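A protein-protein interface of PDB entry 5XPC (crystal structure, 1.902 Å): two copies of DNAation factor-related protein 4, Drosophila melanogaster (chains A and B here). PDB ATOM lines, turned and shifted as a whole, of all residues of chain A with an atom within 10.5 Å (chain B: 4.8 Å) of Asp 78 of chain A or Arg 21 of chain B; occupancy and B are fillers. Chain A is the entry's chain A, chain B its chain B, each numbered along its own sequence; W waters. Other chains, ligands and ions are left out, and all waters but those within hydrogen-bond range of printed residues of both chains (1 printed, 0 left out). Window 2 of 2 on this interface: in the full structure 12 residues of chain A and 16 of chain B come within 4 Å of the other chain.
The backbone carbonyl oxygen (O) of Lys 22 of chain B lies within hydrogen-bond range of the backbone NH (N) of Glu 56 of chain A (2.9 Å).
Among the printed residues, pairs that only touch across the chains: Phe 55 of chain A with Tyr 23 of chain B (3.5 Å), Glu 56 of chain A with Tyr 23 of chain B (3.5 Å), Phe 55 of chain A with Lys 22 of chain B (3.5 Å), Phe 55 of chain A with Val 14 of chain B (3.7 Å) and Asp 78 of chain A with Arg 21 of chain B (3.8 Å).
Of the 22 printed residues of chain A, 3 touch a printed residue of chain B. Printed residues of chain A that touch a printed residue of chain B: Phe 55, Glu 56 and Asp 78. Hydrophobic or aromatic side chains of chain A within 4 Å of the printed part of chain B: Phe 55. Of the 10 printed residues of chain B, 4 touch a printed residue of chain A. Among the printed residues, 6 pairs touch across the chains. Among the printed residues, no Asp or Glu carboxylate lies within 4 Å of a Lys or Arg side-chain nitrogen of the other chain.
No position is printed for both chains. Of the 6 pairs that touch across the chains among the printed residues, none has its exchanged pair printed and touching as well.
Water W1 lies within hydrogen-bond range of NZ of Lys 22 of chain B and O of Asp 53 of chain A.
Of the printed residues of chain B, Phe 55 of chain A touches Val 14, Lys 22 and Tyr 23. Of the printed residues of chain B, Glu 56 of chain A touches Lys 22 and Tyr 23. Gly 76 of chain A touches none of the printed residues of chain B. Val 80 of chain A touches none of the printed residues of chain B. Of the printed residues of chain A, Val 14 of chain B touches Phe 55. Of the printed residues of chain A, Lys 22 of chain B touches Phe 55 (3.5 Å) and Glu 56 (2.9 Å). Of the printed residues of chain A, Tyr 23 of chain B touches Phe 55 (3.5 Å) and Glu 56 (3.5 Å). The nearest residue of chain B that does not touch Asp 78 of chain A is Thr 20 of chain B (4.4 Å).
OD1 of Asp 53 of chain A sits at hydrogen-bond distance from N of Phe 55 of chain A, at 3.2 Å. The guanidinium group (NH1) of Arg 21 of chain B is in hydrogen-bond range of the side-chain hydroxyl (OH) of Tyr 23 of chain B, 2.8 Å away. The backbone carbonyl oxygen (O) of Tyr 23 of chain B sits at hydrogen-bond distance from the backbone NH (N) of Val 14 of chain B (2.9 Å). NH1 of Arg 21 of chain B lies within hydrogen-bond range of O of Lys 40 of chain B. OH of Tyr 49 of chain A sits at hydrogen-bond distance from N of Asp 78 of chain A (3.4 Å). The backbone carbonyl oxygen (O) of Arg 21 of chain B lies within hydrogen-bond range of the side-chain hydroxyl (OG1) of Thr 15 of chain B, at 2.7 Å.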
ATOM      1  N   LEU A  43      22.049  -0.049  -2.378  1.00  0.00           N
ATOM      2  CA  LEU A  43      22.876  -0.214  -1.188  1.00  0.00           C
ATOM      3  C   LEU A  43      24.335   0.013  -1.542  1.00  0.00           C
ATOM      4  O   LEU A  43      24.842  -0.587  -2.492  1.00  0.00           O
ATOM      5  CB  LEU A  43      22.693  -1.613  -0.570  1.00  0.00           C
ATOM      6  CG  LEU A  43      21.274  -1.981  -0.111  1.00  0.00           C
ATOM      7  CD1 LEU A  43      21.029  -3.482  -0.164  1.00  0.00           C
ATOM      8  CD2 LEU A  43      20.991  -1.455   1.289  1.00  0.00           C
ATOM      9  N   GLU A  45      26.952  -0.779   0.351  1.00  0.00           N
ATOM     10  CA  GLU A  45      27.690  -1.968   0.768  1.00  0.00           C
ATOM     11  C   GLU A  45      26.675  -3.062   1.059  1.00  0.00           C
ATOM     12  O   GLU A  45      26.237  -3.234   2.206  1.00  0.00           O
ATOM     13  CB  GLU A  45      28.564  -1.680   1.985  1.00  0.00           C
ATOM     14  CG  GLU A  45      29.092  -0.257   2.041  1.00  0.00           C
ATOM     15  CD  GLU A  45      29.828   0.042   3.334  1.00  0.00           C
ATOM     16  OE1 GLU A  45      29.938  -0.875   4.183  1.00  0.00           O
ATOM     17  OE2 GLU A  45      30.297   1.190   3.518  1.00  0.00           O
ATOM     18  N   PRO A  46      26.260  -3.810   0.040  1.00  0.00           N
ATOM     19  CA  PRO A  46      25.274  -4.870   0.269  1.00  0.00           C
ATOM     20  C   PRO A  46      25.895  -6.054   0.992  1.00  0.00           C
ATOM     21  O   PRO A  46      27.020  -6.464   0.698  1.00  0.00           O
ATOM     22  CB  PRO A  46      24.815  -5.246  -1.147  1.00  0.00           C
ATOM     23  CG  PRO A  46      25.953  -4.864  -2.035  1.00  0.00           C
ATOM     24  CD  PRO A  46      26.572  -3.637  -1.391  1.00  0.00           C
ATOM     25  N   HIS A  47      25.153  -6.576   1.964  1.00  0.00           N
ATOM     26  CA  HIS A  47      25.476  -7.828   2.628  1.00  0.00           C
ATOM     27  C   HIS A  47      24.243  -8.722   2.589  1.00  0.00           C
ATOM     28  O   HIS A  47      23.109  -8.235   2.526  1.00  0.00           O
ATOM     29  CB  HIS A  47      25.924  -7.610   4.085  1.00  0.00           C
ATOM     30  CG  HIS A  47      27.088  -6.683   4.212  1.00  0.00           C
ATOM     31  ND1 HIS A  47      28.254  -7.040   4.856  1.00  0.00           N
ATOM     32  CD2 HIS A  47      27.264  -5.405   3.807  1.00  0.00           C
ATOM     33  CE1 HIS A  47      29.111  -6.037   4.829  1.00  0.00           C
ATOM     34  NE2 HIS A  47      28.534  -5.031   4.196  1.00  0.00           N
ATOM     35  N   LEU A  48      24.462 -10.034   2.610  1.00  0.00           N
ATOM     36  CA  LEU A  48      23.378 -11.010   2.531  1.00  0.00           C
ATOM     37  C   LEU A  48      23.111 -11.617   3.901  1.00  0.00           C
ATOM     38  O   LEU A  48      24.047 -12.020   4.600  1.00  0.00           O
ATOM     39  CB  LEU A  48      23.710 -12.118   1.534  1.00  0.00           C
ATOM     40  CG  LEU A  48      23.776 -11.637   0.081  1.00  0.00           C
ATOM     41  CD1 LEU A  48      24.359 -12.735  -0.766  1.00  0.00           C
ATOM     42  CD2 LEU A  48      22.401 -11.221  -0.461  1.00  0.00           C
ATOM     43  N   TYR A  49      21.831 -11.700   4.269  1.00  0.00           N
ATOM     44  CA  TYR A  49      21.402 -12.284   5.534  1.00  0.00           C
ATOM     45  C   TYR A  49      20.359 -13.362   5.263  1.00  0.00           C
ATOM     46  O   TYR A  49      19.518 -13.205   4.374  1.00  0.00           O
ATOM     47  CB  TYR A  49      20.810 -11.223   6.469  1.00  0.00           C
ATOM     48  CG  TYR A  49      21.719 -10.037   6.750  1.00  0.00           C
ATOM     49  CD1 TYR A  49      21.832  -8.987   5.835  1.00  0.00           C
ATOM     50  CD2 TYR A  49      22.449  -9.964   7.928  1.00  0.00           C
ATOM     51  CE1 TYR A  49      22.650  -7.894   6.090  1.00  0.00           C
ATOM     52  CE2 TYR A  49      23.275  -8.876   8.199  1.00  0.00           C
ATOM     53  CZ  TYR A  49      23.373  -7.846   7.281  1.00  0.00           C
ATOM     54  OH  TYR A  49      24.196  -6.774   7.559  1.00  0.00           O
ATOM     55  N   ASP A  53      16.611 -16.585   9.785  1.00  0.00           N
ATOM     56  CA  ASP A  53      17.020 -16.177  11.123  1.00  0.00           C
ATOM     57  C   ASP A  53      17.967 -14.984  11.162  1.00  0.00           C
ATOM     58  O   ASP A  53      18.466 -14.662  12.240  1.00  0.00           O
ATOM     59  CB  ASP A  53      17.656 -17.365  11.870  1.00  0.00           C
ATOM     60  CG  ASP A  53      18.893 -17.903  11.174  1.00  0.00           C
ATOM     61  OD1 ASP A  53      19.410 -17.236  10.249  1.00  0.00           O
ATOM     62  OD2 ASP A  53      19.362 -18.991  11.572  1.00  0.00           O
ATOM     63  N   GLY A  54      18.239 -14.329  10.032  1.00  0.00           N
ATOM     64  CA  GLY A  54      19.020 -13.105  10.025  1.00  0.00           C
ATOM     65  C   GLY A  54      20.520 -13.273  10.090  1.00  0.00           C
ATOM     66  O   GLY A  54      21.234 -12.268  10.210  1.00  0.00           O
ATOM     67  N   PHE A  55      21.035 -14.494  10.016  1.00  0.00           N
ATOM     68  CA  PHE A  55      22.478 -14.664  10.108  1.00  0.00           C
ATOM     69  C   PHE A  55      23.138 -14.222   8.809  1.00  0.00           C
ATOM     70  O   PHE A  55      22.666 -14.539   7.711  1.00  0.00           O
ATOM     71  CB  PHE A  55      22.827 -16.110  10.473  1.00  0.00           C
ATOM     72  CG  PHE A  55      22.776 -16.353  11.950  1.00  0.00           C
ATOM     73  CD1 PHE A  55      21.559 -16.329  12.619  1.00  0.00           C
ATOM     74  CD2 PHE A  55      23.946 -16.521  12.690  1.00  0.00           C
ATOM     75  CE1 PHE A  55      21.505 -16.499  13.997  1.00  0.00           C
ATOM     76  CE2 PHE A  55      23.895 -16.686  14.068  1.00  0.00           C
ATOM     77  CZ  PHE A  55      22.675 -16.670  14.723  1.00  0.00           C
ATOM     78  N   GLU A  56      24.194 -13.425   8.938  1.00  0.00           N
ATOM     79  CA  GLU A  56      24.837 -12.846   7.769  1.00  0.00           C
ATOM     80  C   GLU A  56      25.738 -13.878   7.111  1.00  0.00           C
ATOM     81  O   GLU A  56      26.452 -14.621   7.788  1.00  0.00           O
ATOM     82  CB  GLU A  56      25.657 -11.605   8.152  1.00  0.00           C
ATOM     83  CG  GLU A  56      26.398 -11.013   6.946  1.00  0.00           C
ATOM     84  CD  GLU A  56      27.219  -9.788   7.266  1.00  0.00           C
ATOM     85  OE1 GLU A  56      26.999  -9.180   8.334  1.00  0.00           O
ATOM     86  OE2 GLU A  56      28.084  -9.430   6.434  1.00  0.00           O
ATOM     87  N   VAL A  57      25.705 -13.925   5.781  1.00  0.00           N
ATOM     88  CA  VAL A  57      26.559 -14.831   5.016  1.00  0.00           C
ATOM     89  C   VAL A  57      27.947 -14.198   4.993  1.00  0.00           C
ATOM     90  O   VAL A  57      28.213 -13.288   4.204  1.00  0.00           O
ATOM     91  CB  VAL A  57      26.014 -15.070   3.608  1.00  0.00           C
ATOM     92  CG1 VAL A  57      26.895 -16.047   2.849  1.00  0.00           C
ATOM     93  CG2 VAL A  57      24.588 -15.598   3.690  1.00  0.00           C
ATOM     94  N   SER A  58      28.835 -14.655   5.878  1.00  0.00           N
ATOM     95  CA  SER A  58      30.087 -13.935   6.082  1.00  0.00           C
ATOM     96  C   SER A  58      31.181 -14.321   5.093  1.00  0.00           C
ATOM     97  O   SER A  58      32.107 -13.528   4.880  1.00  0.00           O
ATOM     98  CB  SER A  58      30.599 -14.128   7.517  1.00  0.00           C
ATOM     99  OG  SER A  58      31.261 -15.380   7.679  1.00  0.00           O
ATOM    100  N   ILE A  73      17.886 -11.978   2.545  1.00  0.00           N
ATOM    101  CA  ILE A  73      17.564 -10.558   2.597  1.00  0.00           C
ATOM    102  C   ILE A  73      18.853  -9.804   2.329  1.00  0.00           C
ATOM    103  O   ILE A  73      19.867 -10.060   2.984  1.00  0.00           O
ATOM    104  CB  ILE A  73      16.993 -10.155   3.970  1.00  0.00           C
ATOM    105  CG1 ILE A  73      15.857 -11.079   4.422  1.00  0.00           C
ATOM    106  CG2 ILE A  73      16.560  -8.697   3.952  1.00  0.00           C
ATOM    107  CD1 ILE A  73      14.714 -11.164   3.468  1.00  0.00           C
ATOM    108  N   VAL A  74      18.835  -8.882   1.376  1.00  0.00           N
ATOM    109  CA  VAL A  74      19.995  -8.029   1.144  1.00  0.00           C
ATOM    110  C   VAL A  74      19.761  -6.703   1.855  1.00  0.00           C
ATOM    111  O   VAL A  74      18.653  -6.152   1.815  1.00  0.00           O
ATOM    112  CB  VAL A  74      20.272  -7.833  -0.358  1.00  0.00           C
ATOM    113  CG1 VAL A  74      19.137  -7.092  -1.035  1.00  0.00           C
ATOM    114  CG2 VAL A  74      21.607  -7.101  -0.555  1.00  0.00           C
ATOM    115  N   SER A  75      20.782  -6.218   2.554  1.00  0.00           N
ATOM    116  CA  SER A  75      20.691  -4.947   3.263  1.00  0.00           C
ATOM    117  C   SER A  75      22.111  -4.441   3.482  1.00  0.00           C
ATOM    118  O   SER A  75      23.079  -5.015   2.974  1.00  0.00           O
ATOM    119  CB  SER A  75      19.913  -5.103   4.575  1.00  0.00           C
ATOM    120  OG  SER A  75      19.673  -3.841   5.190  1.00  0.00           O
ATOM    121  N   GLY A  76      22.235  -3.350   4.237  1.00  0.00           N
ATOM    122  CA  GLY A  76      23.532  -2.776   4.509  1.00  0.00           C
ATOM    123  C   GLY A  76      24.236  -3.501   5.640  1.00  0.00           C
ATOM    124  O   GLY A  76      23.744  -4.509   6.156  1.00  0.00           O
ATOM    125  N   PRO A  77      25.401  -2.999   6.052  1.00  0.00           N
ATOM    126  CA  PRO A  77      26.120  -3.630   7.168  1.00  0.00           C
ATOM    127  C   PRO A  77      25.414  -3.394   8.493  1.00  0.00           C
ATOM    128  O   PRO A  77      24.726  -2.387   8.688  1.00  0.00           O
ATOM    129  CB  PRO A  77      27.497  -2.951   7.152  1.00  0.00           C
ATOM    130  CG  PRO A  77      27.364  -1.737   6.286  1.00  0.00           C
ATOM    131  CD  PRO A  77      26.026  -1.743   5.600  1.00  0.00           C
ATOM    132  N   ASP A  78      25.606  -4.336   9.417  1.00  0.00           N
ATOM    133  CA  ASP A  78      24.978  -4.284  10.737  1.00  0.00           C
ATOM    134  C   ASP A  78      23.479  -4.011  10.606  1.00  0.00           C
ATOM    135  O   ASP A  78      22.908  -3.161  11.292  1.00  0.00           O
ATOM    136  CB  ASP A  78      25.658  -3.236  11.621  1.00  0.00           C
ATOM    137  CG  ASP A  78      25.400  -3.459  13.098  1.00  0.00           C
ATOM    138  OD1 ASP A  78      24.746  -4.466  13.447  1.00  0.00           O
ATOM    139  OD2 ASP A  78      25.861  -2.630  13.911  1.00  0.00           O
ATOM    140  N   ALA A  79      22.840  -4.747   9.700  1.00  0.00           N
ATOM    141  CA  ALA A  79      21.479  -4.426   9.296  1.00  0.00           C
ATOM    142  C   ALA A  79      20.463  -4.849  10.351  1.00  0.00           C
ATOM    143  O   ALA A  79      20.696  -5.772  11.139  1.00  0.00           O
ATOM    144  CB  ALA A  79      21.149  -5.095   7.964  1.00  0.00           C
ATOM    145  N   VAL A  80      19.332  -4.147  10.366  1.00  0.00           N
ATOM    146  CA  VAL A  80      18.157  -4.576  11.117  1.00  0.00           C
ATOM    147  C   VAL A  80      17.278  -5.372  10.156  1.00  0.00           C
ATOM    148  O   VAL A  80      16.654  -4.808   9.252  1.00  0.00           O
ATOM    149  CB  VAL A  80      17.400  -3.391  11.725  1.00  0.00           C
ATOM    150  CG1 VAL A  80      16.160  -3.882  12.471  1.00  0.00           C
ATOM    151  CG2 VAL A  80      18.303  -2.618  12.663  1.00  0.00           C
ATOM    152  N   ILE A  81      17.249  -6.690  10.340  1.00  0.00           N
ATOM    153  CA  ILE A  81      16.569  -7.616   9.438  1.00  0.00           C
ATOM    154  C   ILE A  81      15.320  -8.130  10.141  1.00  0.00           C
ATOM    155  O   ILE A  81      15.388  -8.560  11.299  1.00  0.00           O
ATOM    156  CB  ILE A  81      17.496  -8.780   9.039  1.00  0.00           C
ATOM    157  CG1 ILE A  81      18.698  -8.263   8.248  1.00  0.00           C
ATOM    158  CG2 ILE A  81      16.752  -9.840   8.249  1.00  0.00           C
ATOM    159  CD1 ILE A  81      18.325  -7.330   7.107  1.00  0.00           C
ATOM    160  N   THR A  82      14.181  -8.071   9.456  1.00  0.00           N
ATOM    161  CA  THR A  82      12.967  -8.737   9.923  1.00  0.00           C
ATOM    162  C   THR A  82      12.995 -10.173   9.414  1.00  0.00           C
ATOM    163  O   THR A  82      12.815 -10.420   8.220  1.00  0.00           O
ATOM    164  CB  THR A  82      11.710  -8.016   9.443  1.00  0.00           C
ATOM    165  OG1 THR A  82      11.789  -6.624   9.789  1.00  0.00           O
ATOM    166  CG2 THR A  82      10.485  -8.629  10.106  1.00  0.00           C
ATOM    167  N   VAL B  14      27.374 -18.308  14.462  1.00  0.00           N
ATOM    168  CA  VAL B  14      28.060 -17.748  15.626  1.00  0.00           C
ATOM    169  C   VAL B  14      27.468 -16.385  15.942  1.00  0.00           C
ATOM    170  O   VAL B  14      27.303 -15.543  15.047  1.00  0.00           O
ATOM    171  CB  VAL B  14      29.578 -17.624  15.392  1.00  0.00           C
ATOM    172  CG1 VAL B  14      30.273 -16.973  16.611  1.00  0.00           C
ATOM    173  CG2 VAL B  14      30.187 -18.990  15.093  1.00  0.00           C
ATOM    174  N   THR B  15      27.162 -16.159  17.216  1.00  0.00           N
ATOM    175  CA  THR B  15      26.768 -14.845  17.684  1.00  0.00           C
ATOM    176  C   THR B  15      27.422 -14.626  19.040  1.00  0.00           C
ATOM    177  O   THR B  15      28.102 -15.510  19.575  1.00  0.00           O
ATOM    178  CB  THR B  15      25.229 -14.727  17.722  1.00  0.00           C
ATOM    179  OG1 THR B  15      24.837 -13.375  17.986  1.00  0.00           O
ATOM    180  CG2 THR B  15      24.626 -15.689  18.765  1.00  0.00           C
ATOM    181  N   ASP B  16      27.251 -13.434  19.590  1.00  0.00           N
ATOM    182  CA  ASP B  16      27.786 -13.150  20.910  1.00  0.00           C
ATOM    183  C   ASP B  16      26.689 -13.355  21.952  1.00  0.00           C
ATOM    184  O   ASP B  16      25.552 -13.722  21.638  1.00  0.00           O
ATOM    185  CB  ASP B  16      28.403 -11.748  20.975  1.00  0.00           C
ATOM    186  CG  ASP B  16      27.444 -10.643  20.556  1.00  0.00           C
ATOM    187  OD1 ASP B  16      26.222 -10.877  20.479  1.00  0.00           O
ATOM    188  OD2 ASP B  16      27.927  -9.514  20.320  1.00  0.00           O
ATOM    189  N   ARG B  19      23.558 -11.473  21.338  1.00  0.00           N
ATOM    190  CA  ARG B  19      22.913 -11.676  20.040  1.00  0.00           C
ATOM    191  C   ARG B  19      22.860 -10.376  19.237  1.00  0.00           C
ATOM    192  O   ARG B  19      21.878 -10.088  18.551  1.00  0.00           O
ATOM    193  CB  ARG B  19      21.511 -12.275  20.203  1.00  0.00           C
ATOM    194  CG  ARG B  19      21.470 -13.787  20.425  1.00  0.00           C
ATOM    195  CD  ARG B  19      21.924 -14.192  21.833  1.00  0.00           C
ATOM    196  NE  ARG B  19      21.599 -15.592  22.125  1.00  0.00           N
ATOM    197  CZ  ARG B  19      21.982 -16.244  23.221  1.00  0.00           C
ATOM    198  NH1 ARG B  19      22.718 -15.631  24.143  1.00  0.00           N
ATOM    199  NH2 ARG B  19      21.637 -17.514  23.393  1.00  0.00           N
ATOM    200  N   THR B  20      23.933  -9.584  19.320  1.00  0.00           N
ATOM    201  CA  THR B  20      23.952  -8.264  18.689  1.00  0.00           C
ATOM    202  C   THR B  20      24.235  -8.358  17.197  1.00  0.00           C
ATOM    203  O   THR B  20      23.665  -7.598  16.406  1.00  0.00           O
ATOM    204  CB  THR B  20      25.008  -7.368  19.332  1.00  0.00           C
ATOM    205  OG1 THR B  20      26.312  -7.911  19.075  1.00  0.00           O
ATOM    206  CG2 THR B  20      24.779  -7.224  20.836  1.00  0.00           C
ATOM    207  N   ARG B  21      25.146  -9.247  16.811  1.00  0.00           N
ATOM    208  CA  ARG B  21      25.488  -9.506  15.422  1.00  0.00           C
ATOM    209  C   ARG B  21      25.554 -11.011  15.228  1.00  0.00           C
ATOM    210  O   ARG B  21      25.958 -11.748  16.136  1.00  0.00           O
ATOM    211  CB  ARG B  21      26.820  -8.842  15.032  1.00  0.00           C
ATOM    212  CG  ARG B  21      26.717  -7.321  14.892  1.00  0.00           C
ATOM    213  CD  ARG B  21      28.073  -6.650  14.699  1.00  0.00           C
ATOM    214  NE  ARG B  21      28.949  -6.793  15.861  1.00  0.00           N
ATOM    215  CZ  ARG B  21      30.139  -7.385  15.833  1.00  0.00           C
ATOM    216  NH1 ARG B  21      30.605  -7.888  14.695  1.00  0.00           N
ATOM    217  NH2 ARG B  21      30.874  -7.462  16.941  1.00  0.00           N
ATOM    218  N   LYS B  22      25.136 -11.466  14.048  1.00  0.00           N
ATOM    219  CA  LYS B  22      24.936 -12.886  13.775  1.00  0.00           C
ATOM    220  C   LYS B  22      25.613 -13.231  12.461  1.00  0.00           C
ATOM    221  O   LYS B  22      25.337 -12.599  11.438  1.00  0.00           O
ATOM    222  CB  LYS B  22      23.438 -13.216  13.708  1.00  0.00           C
ATOM    223  CG  LYS B  22      22.661 -12.732  14.917  1.00  0.00           C
ATOM    224  CD  LYS B  22      21.182 -13.055  14.821  1.00  0.00           C
ATOM    225  CE  LYS B  22      20.423 -12.386  15.959  1.00  0.00           C
ATOM    226  NZ  LYS B  22      19.121 -13.046  16.248  1.00  0.00           N
ATOM    227  N   TYR B  23      26.508 -14.214  12.485  1.00  0.00           N
ATOM    228  CA  TYR B  23      27.267 -14.569  11.298  1.00  0.00           C
ATOM    229  C   TYR B  23      27.159 -16.055  11.016  1.00  0.00           C
ATOM    230  O   TYR B  23      27.301 -16.879  11.926  1.00  0.00           O
ATOM    231  CB  TYR B  23      28.740 -14.198  11.445  1.00  0.00           C
ATOM    232  CG  TYR B  23      28.955 -12.728  11.640  1.00  0.00           C
ATOM    233  CD1 TYR B  23      29.123 -12.194  12.915  1.00  0.00           C
ATOM    234  CD2 TYR B  23      28.966 -11.862  10.553  1.00  0.00           C
ATOM    235  CE1 TYR B  23      29.314 -10.833  13.095  1.00  0.00           C
ATOM    236  CE2 TYR B  23      29.161 -10.505  10.727  1.00  0.00           C
ATOM    237  CZ  TYR B  23      29.332  -9.998  12.000  1.00  0.00           C
ATOM    238  OH  TYR B  23      29.521  -8.642  12.175  1.00  0.00           O
ATOM    239  N   LYS B  40      35.273 -11.264  13.783  1.00  0.00           N
ATOM    240  CA  LYS B  40      34.000 -10.557  13.889  1.00  0.00           C
ATOM    241  C   LYS B  40      33.717 -10.043  15.299  1.00  0.00           C
ATOM    242  O   LYS B  40      33.080  -8.990  15.448  1.00  0.00           O
ATOM    243  CB  LYS B  40      32.862 -11.480  13.434  1.00  0.00           C
ATOM    244  CG  LYS B  40      32.904 -11.821  11.933  1.00  0.00           C
ATOM    245  CD  LYS B  40      32.829 -10.550  11.097  1.00  0.00           C
ATOM    246  CE  LYS B  40      32.595 -10.827   9.603  1.00  0.00           C
ATOM    247  NZ  LYS B  40      33.698 -11.617   9.003  1.00  0.00           N
ATOM    248  N   PHE B  41      34.177 -10.760  16.330  1.00  0.00           N
ATOM    249  CA  PHE B  41      33.990 -10.406  17.740  1.00  0.00           C
ATOM    250  C   PHE B  41      35.354 -10.351  18.411  1.00  0.00           C
ATOM    251  O   PHE B  41      35.859 -11.382  18.889  1.00  0.00           O
ATOM    252  CB  PHE B  41      33.105 -11.423  18.460  1.00  0.00           C
ATOM    253  CG  PHE B  41      31.759 -11.620  17.814  1.00  0.00           C
ATOM    254  CD1 PHE B  41      30.704 -10.761  18.105  1.00  0.00           C
ATOM    255  CD2 PHE B  41      31.550 -12.660  16.926  1.00  0.00           C
ATOM    256  CE1 PHE B  41      29.446 -10.933  17.512  1.00  0.00           C
ATOM    257  CE2 PHE B  41      30.294 -12.844  16.331  1.00  0.00           C
ATOM    258  CZ  PHE B  41      29.249 -11.974  16.629  1.00  0.00           C
HETATM  259  O   HOH W   1      17.981 -14.708  14.742  1.00  0.00           O
